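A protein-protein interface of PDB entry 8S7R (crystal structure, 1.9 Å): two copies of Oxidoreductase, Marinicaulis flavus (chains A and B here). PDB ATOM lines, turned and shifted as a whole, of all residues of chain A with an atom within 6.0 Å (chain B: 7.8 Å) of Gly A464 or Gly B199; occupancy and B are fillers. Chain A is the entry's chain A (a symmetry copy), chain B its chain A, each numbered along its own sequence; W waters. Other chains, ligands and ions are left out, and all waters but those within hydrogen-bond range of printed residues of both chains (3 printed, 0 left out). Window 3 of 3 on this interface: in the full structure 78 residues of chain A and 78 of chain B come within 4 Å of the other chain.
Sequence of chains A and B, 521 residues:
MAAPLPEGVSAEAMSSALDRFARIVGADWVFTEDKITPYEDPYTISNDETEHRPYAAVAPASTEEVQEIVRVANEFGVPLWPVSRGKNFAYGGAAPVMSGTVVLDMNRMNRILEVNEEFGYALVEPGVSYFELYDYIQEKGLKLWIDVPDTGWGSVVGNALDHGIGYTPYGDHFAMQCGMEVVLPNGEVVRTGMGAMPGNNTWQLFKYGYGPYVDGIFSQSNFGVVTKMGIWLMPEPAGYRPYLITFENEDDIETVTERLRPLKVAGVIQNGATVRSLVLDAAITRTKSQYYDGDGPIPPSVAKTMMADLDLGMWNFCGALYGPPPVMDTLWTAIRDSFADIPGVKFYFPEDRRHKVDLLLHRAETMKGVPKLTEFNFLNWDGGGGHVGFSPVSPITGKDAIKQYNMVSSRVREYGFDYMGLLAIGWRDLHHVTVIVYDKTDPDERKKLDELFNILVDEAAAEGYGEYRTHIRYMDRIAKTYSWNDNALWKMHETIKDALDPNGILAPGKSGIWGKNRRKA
The side-chain amide nitrogen (ND2) of Asn B200 lies within hydrogen-bond range of the backbone carbonyl oxygen (O) of Met B194 (3.2 Å). The side-chain amide nitrogen (ND2) of Asn B200 sits at hydrogen-bond distance from the backbone carbonyl oxygen (O) of Met B197. The backbone NH (N) of Thr B202 lies within hydrogen-bond range of the side-chain amide oxygen (OD1) of Asn B200, at 3.1 Å. N of Val A393 sits at hydrogen-bond distance from O of Gly A466, 2.8 Å away. O of Ala A460 lies within hydrogen-bond range of N of Tyr A465, at 3.0 Å.
Printed residues of chain A that touch a printed residue of chain B: Ser A394, Ala A461, Gly A464, Tyr A465 and Gly A466. Hydrophobic or aromatic side chains of chain A that line the printed part of chain B: Ala A461. Of the 10 printed residues of chain B, 5 touch a printed residue of chain A. Hydrophobic or aromatic side chains of chain B within 4 Å of the printed part of chain A: Met B194 and Met B197. Among the printed residues, 8 pairs touch across the chains.
SD of Met B197 lies within hydrogen-bond range of N of Gly A466 (3.5 Å).
Among the printed residues, pairs that only touch across the chains: Ser A394 with Thr B202, Ala A461 with Met B197, Gly A464 with Met B197, Gly A464 with Gly B199, Gly A464 with Asn B200, Tyr A465 with Met B197 and Gly A466 with Met B194.
Gly A464 touches just these residues of chain B: Met B197, Gly B199 and Asn B200. Printed residues of chain B within 4 Å of Tyr A465: Met B197. Of the printed residues of chain B, Gly A466 touches Met B194 (3.9 Å) and Met B197 (3.5 Å). Of the printed residues of chain A, Met B194 touches Gly A466. Gly B195 touches none of the printed residues of chain A. Pro B198 touches none of the printed residues of chain A. Of chain A, only Gly A464 comes within 4 Å of Gly B199. Printed residues of chain A within 4 Å of Thr B202: Ser A394 (3.6 Å). The nearest residue of chain B that does not touch Gly A464 is Asn B201 (4.5 Å).
No position is printed for both chains. Of the 8 pairs that touch across the chains among the printed residues, none has its exchanged pair printed and touching as well.
Water W2 lies within hydrogen-bond range of O of Gly A464 (2.6 Å), O of Val A393 (2.7 Å), OG1 of Thr B202 (2.8 Å) and N of Gly A466 (3.3 Å). Water W1 bridges the side-chain amide nitrogen of Asn B201 (2.8 Å) and the backbone carbonyl oxygen of Glu A463 (2.9 Å). Water W3 bridges the backbone NH (N) of Asn B201 (2.9 Å) and the backbone carbonyl oxygen (O) of Gly A464 (3.0 Å).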
ATOM      1  N   VAL A 393     -11.320 -11.253  -8.591  1.00  0.00           N
ATOM      2  CA  VAL A 393     -11.243 -12.022  -9.821  1.00  0.00           C
ATOM      3  C   VAL A 393     -10.407 -11.264 -10.837  1.00  0.00           C
ATOM      4  O   VAL A 393     -10.597 -10.079 -10.986  1.00  0.00           O
ATOM      5  CB  VAL A 393     -12.641 -12.246 -10.419  1.00  0.00           C
ATOM      6  CG1 VAL A 393     -12.592 -13.305 -11.487  1.00  0.00           C
ATOM      7  CG2 VAL A 393     -13.664 -12.603  -9.358  1.00  0.00           C
ATOM      8  N   SER A 394      -9.635 -11.999 -11.636  1.00  0.00           N
ATOM      9  CA  SER A 394      -8.831 -11.455 -12.708  1.00  0.00           C
ATOM     10  C   SER A 394      -8.675 -12.509 -13.799  1.00  0.00           C
ATOM     11  O   SER A 394      -8.992 -13.678 -13.588  1.00  0.00           O
ATOM     12  CB  SER A 394      -7.482 -10.995 -12.189  1.00  0.00           C
ATOM     13  OG  SER A 394      -6.748 -12.095 -11.665  1.00  0.00           O
ATOM     14  N   GLU A 459      -7.424   0.087  -5.021  1.00  0.00           N
ATOM     15  CA  GLU A 459      -6.411   0.024  -6.052  1.00  0.00           C
ATOM     16  C   GLU A 459      -6.623  -1.175  -6.975  1.00  0.00           C
ATOM     17  O   GLU A 459      -6.370  -1.094  -8.170  1.00  0.00           O
ATOM     18  CB  GLU A 459      -5.029   0.028  -5.391  1.00  0.00           C
ATOM     19  CG  GLU A 459      -4.700   1.409  -4.883  1.00  0.00           C
ATOM     20  CD  GLU A 459      -3.378   1.606  -4.181  1.00  0.00           C
ATOM     21  OE1 GLU A 459      -2.648   0.628  -3.981  1.00  0.00           O
ATOM     22  OE2 GLU A 459      -3.125   2.755  -3.768  1.00  0.00           O
ATOM     23  N   ALA A 460      -7.068  -2.297  -6.417  1.00  0.00           N
ATOM     24  CA  ALA A 460      -7.419  -3.460  -7.224  1.00  0.00           C
ATOM     25  C   ALA A 460      -8.578  -3.165  -8.190  1.00  0.00           C
ATOM     26  O   ALA A 460      -8.590  -3.594  -9.348  1.00  0.00           O
ATOM     27  CB  ALA A 460      -7.787  -4.594  -6.295  1.00  0.00           C
ATOM     28  N   ALA A 461      -9.610  -2.498  -7.683  1.00  0.00           N
ATOM     29  CA  ALA A 461     -10.795  -2.228  -8.479  1.00  0.00           C
ATOM     30  C   ALA A 461     -10.458  -1.318  -9.663  1.00  0.00           C
ATOM     31  O   ALA A 461     -11.011  -1.493 -10.748  1.00  0.00           O
ATOM     32  CB  ALA A 461     -11.874  -1.639  -7.614  1.00  0.00           C
ATOM     33  N   ALA A 462      -9.542  -0.361  -9.462  1.00  0.00           N
ATOM     34  CA  ALA A 462      -9.104   0.513 -10.551  1.00  0.00           C
ATOM     35  C   ALA A 462      -8.374  -0.265 -11.653  1.00  0.00           C
ATOM     36  O   ALA A 462      -8.378   0.167 -12.801  1.00  0.00           O
ATOM     37  CB  ALA A 462      -8.238   1.629 -10.010  1.00  0.00           C
ATOM     38  N   GLU A 463      -7.778  -1.430 -11.341  1.00  0.00           N
ATOM     39  CA  GLU A 463      -7.188  -2.283 -12.367  1.00  0.00           C
ATOM     40  C   GLU A 463      -8.197  -3.271 -12.952  1.00  0.00           C
ATOM     41  O   GLU A 463      -7.825  -4.100 -13.765  1.00  0.00           O
ATOM     42  CB  GLU A 463      -6.033  -3.122 -11.818  1.00  0.00           C
ATOM     43  CG  GLU A 463      -4.911  -2.327 -11.229  1.00  0.00           C
ATOM     44  CD  GLU A 463      -4.372  -1.256 -12.160  1.00  0.00           C
ATOM     45  OE1 GLU A 463      -4.030  -1.601 -13.298  1.00  0.00           O
ATOM     46  OE2 GLU A 463      -4.279  -0.093 -11.728  1.00  0.00           O
ATOM     47  N   GLY A 464      -9.464  -3.200 -12.551  1.00  0.00           N
ATOM     48  CA  GLY A 464     -10.494  -4.104 -13.060  1.00  0.00           C
ATOM     49  C   GLY A 464     -10.644  -5.438 -12.306  1.00  0.00           C
ATOM     50  O   GLY A 464     -11.307  -6.367 -12.798  1.00  0.00           O
ATOM     51  N   TYR A 465     -10.117  -5.509 -11.078  1.00  0.00           N
ATOM     52  CA  TYR A 465     -10.206  -6.729 -10.279  1.00  0.00           C
ATOM     53  C   TYR A 465     -11.213  -6.539  -9.154  1.00  0.00           C
ATOM     54  O   TYR A 465     -10.973  -5.768  -8.224  1.00  0.00           O
ATOM     55  CB  TYR A 465      -8.832  -7.063  -9.713  1.00  0.00           C
ATOM     56  CG  TYR A 465      -7.682  -7.054 -10.690  1.00  0.00           C
ATOM     57  CD1 TYR A 465      -7.758  -7.682 -11.924  1.00  0.00           C
ATOM     58  CD2 TYR A 465      -6.473  -6.447 -10.351  1.00  0.00           C
ATOM     59  CE1 TYR A 465      -6.691  -7.671 -12.814  1.00  0.00           C
ATOM     60  CE2 TYR A 465      -5.394  -6.446 -11.225  1.00  0.00           C
ATOM     61  CZ  TYR A 465      -5.491  -7.082 -12.447  1.00  0.00           C
ATOM     62  OH  TYR A 465      -4.394  -7.066 -13.280  1.00  0.00           O
ATOM     63  N   GLY A 466     -12.352  -7.239  -9.234  1.00  0.00           N
ATOM     64  CA  GLY A 466     -13.404  -7.112  -8.244  1.00  0.00           C
ATOM     65  C   GLY A 466     -13.519  -8.330  -7.315  1.00  0.00           C
ATOM     66  O   GLY A 466     -13.357  -9.454  -7.751  1.00  0.00           O
ATOM     67  N   ARG B 191     -26.137  -5.300 -16.335  1.00  0.00           N
ATOM     68  CA  ARG B 191     -25.209  -6.374 -16.643  1.00  0.00           C
ATOM     69  C   ARG B 191     -24.969  -7.176 -15.370  1.00  0.00           C
ATOM     70  O   ARG B 191     -24.819  -6.601 -14.281  1.00  0.00           O
ATOM     71  CB  ARG B 191     -23.898  -5.790 -17.181  1.00  0.00           C
ATOM     72  CG  ARG B 191     -24.080  -5.040 -18.492  1.00  0.00           C
ATOM     73  CD  ARG B 191     -22.780  -4.523 -19.113  1.00  0.00           C
ATOM     74  NE  ARG B 191     -23.013  -3.970 -20.436  1.00  0.00           N
ATOM     75  CZ  ARG B 191     -22.055  -3.576 -21.267  1.00  0.00           C
ATOM     76  NH1 ARG B 191     -20.797  -3.591 -20.863  1.00  0.00           N
ATOM     77  NH2 ARG B 191     -22.356  -3.127 -22.477  1.00  0.00           N
ATOM     78  N   MET B 194     -19.559 -10.128 -13.371  1.00  0.00           N
ATOM     79  CA  MET B 194     -18.410  -9.235 -13.398  1.00  0.00           C
ATOM     80  C   MET B 194     -18.686  -8.070 -14.351  1.00  0.00           C
ATOM     81  O   MET B 194     -18.093  -7.009 -14.196  1.00  0.00           O
ATOM     82  CB  MET B 194     -17.135  -9.975 -13.823  1.00  0.00           C
ATOM     83  CG  MET B 194     -16.643 -11.038 -12.841  1.00  0.00           C
ATOM     84  SD  MET B 194     -16.699 -10.596 -11.070  1.00  0.00           S
ATOM     85  CE  MET B 194     -15.552  -9.232 -11.005  1.00  0.00           C
ATOM     86  N   GLY B 195     -19.694  -8.210 -15.242  1.00  0.00           N
ATOM     87  CA  GLY B 195     -20.085  -7.125 -16.122  1.00  0.00           C
ATOM     88  C   GLY B 195     -20.620  -5.873 -15.430  1.00  0.00           C
ATOM     89  O   GLY B 195     -20.624  -4.798 -16.023  1.00  0.00           O
ATOM     90  N   ALA B 196     -21.092  -6.004 -14.185  1.00  0.00           N
ATOM     91  CA  ALA B 196     -21.543  -4.862 -13.412  1.00  0.00           C
ATOM     92  C   ALA B 196     -20.375  -4.055 -12.864  1.00  0.00           C
ATOM     93  O   ALA B 196     -20.581  -2.983 -12.329  1.00  0.00           O
ATOM     94  CB  ALA B 196     -22.422  -5.327 -12.300  1.00  0.00           C
ATOM     95  N   MET B 197     -19.145  -4.556 -12.997  1.00  0.00           N
ATOM     96  CA  MET B 197     -17.983  -3.781 -12.621  1.00  0.00           C
ATOM     97  C   MET B 197     -17.371  -3.103 -13.849  1.00  0.00           C
ATOM     98  O   MET B 197     -16.822  -3.766 -14.725  1.00  0.00           O
ATOM     99  CB  MET B 197     -16.909  -4.677 -11.999  1.00  0.00           C
ATOM    100  CG  MET B 197     -15.615  -3.940 -11.830  1.00  0.00           C
ATOM    101  SD  MET B 197     -14.408  -4.939 -10.957  1.00  0.00           S
ATOM    102  CE  MET B 197     -13.402  -3.605 -10.333  1.00  0.00           C
ATOM    103  N   PRO B 198     -17.336  -1.756 -13.918  1.00  0.00           N
ATOM    104  CA  PRO B 198     -16.744  -1.080 -15.064  1.00  0.00           C
ATOM    105  C   PRO B 198     -15.268  -1.438 -15.148  1.00  0.00           C
ATOM    106  O   PRO B 198     -14.618  -1.504 -14.116  1.00  0.00           O
ATOM    107  CB  PRO B 198     -16.945   0.409 -14.732  1.00  0.00           C
ATOM    108  CG  PRO B 198     -18.061   0.421 -13.739  1.00  0.00           C
ATOM    109  CD  PRO B 198     -17.824  -0.815 -12.901  1.00  0.00           C
ATOM    110  N   GLY B 199     -14.782  -1.722 -16.352  1.00  0.00           N
ATOM    111  CA  GLY B 199     -13.366  -1.955 -16.613  1.00  0.00           C
ATOM    112  C   GLY B 199     -12.912  -3.393 -16.338  1.00  0.00           C
ATOM    113  O   GLY B 199     -11.716  -3.670 -16.341  1.00  0.00           O
ATOM    114  N   ASN B 200     -13.851  -4.306 -16.039  1.00  0.00           N
ATOM    115  CA  ASN B 200     -13.516  -5.712 -15.872  1.00  0.00           C
ATOM    116  C   ASN B 200     -12.999  -6.283 -17.197  1.00  0.00           C
ATOM    117  O   ASN B 200     -13.356  -5.805 -18.272  1.00  0.00           O
ATOM    118  CB  ASN B 200     -14.730  -6.544 -15.430  1.00  0.00           C
ATOM    119  CG  ASN B 200     -15.708  -6.765 -16.571  1.00  0.00           C
ATOM    120  OD1 ASN B 200     -15.585  -7.748 -17.294  1.00  0.00           O
ATOM    121  ND2 ASN B 200     -16.633  -5.830 -16.790  1.00  0.00           N
ATOM    122  N   ASN B 201     -12.225  -7.374 -17.112  1.00  0.00           N
ATOM    123  CA  ASN B 201     -11.900  -8.208 -18.251  1.00  0.00           C
ATOM    124  C   ASN B 201     -12.307  -9.644 -17.924  1.00  0.00           C
ATOM    125  O   ASN B 201     -11.738 -10.587 -18.475  1.00  0.00           O
ATOM    126  CB  ASN B 201     -10.410  -8.092 -18.576  1.00  0.00           C
ATOM    127  CG  ASN B 201     -10.083  -6.767 -19.235  1.00  0.00           C
ATOM    128  OD1 ASN B 201     -10.539  -6.498 -20.335  1.00  0.00           O
ATOM    129  ND2 ASN B 201      -9.311  -5.927 -18.572  1.00  0.00           N
ATOM    130  N   THR B 202     -13.304  -9.777 -17.044  1.00  0.00           N
ATOM    131  CA  THR B 202     -13.701 -11.042 -16.442  1.00  0.00           C
ATOM    132  C   THR B 202     -15.188 -11.376 -16.619  1.00  0.00           C
ATOM    133  O   THR B 202     -15.635 -12.364 -16.035  1.00  0.00           O
ATOM    134  CB  THR B 202     -13.321 -11.037 -14.949  1.00  0.00           C
ATOM    135  OG1 THR B 202     -13.894  -9.868 -14.362  1.00  0.00           O
ATOM    136  CG2 THR B 202     -11.821 -11.040 -14.766  1.00  0.00           C
HETATM  137  O   HOH W   1      -8.699  -6.012 -15.832  1.00  0.00           O
HETATM  138  O   HOH W   2     -12.505  -8.608 -12.233  1.00  0.00           O
HETATM  139  O   HOH W   3     -10.323  -7.988 -15.075  1.00  0.00           O
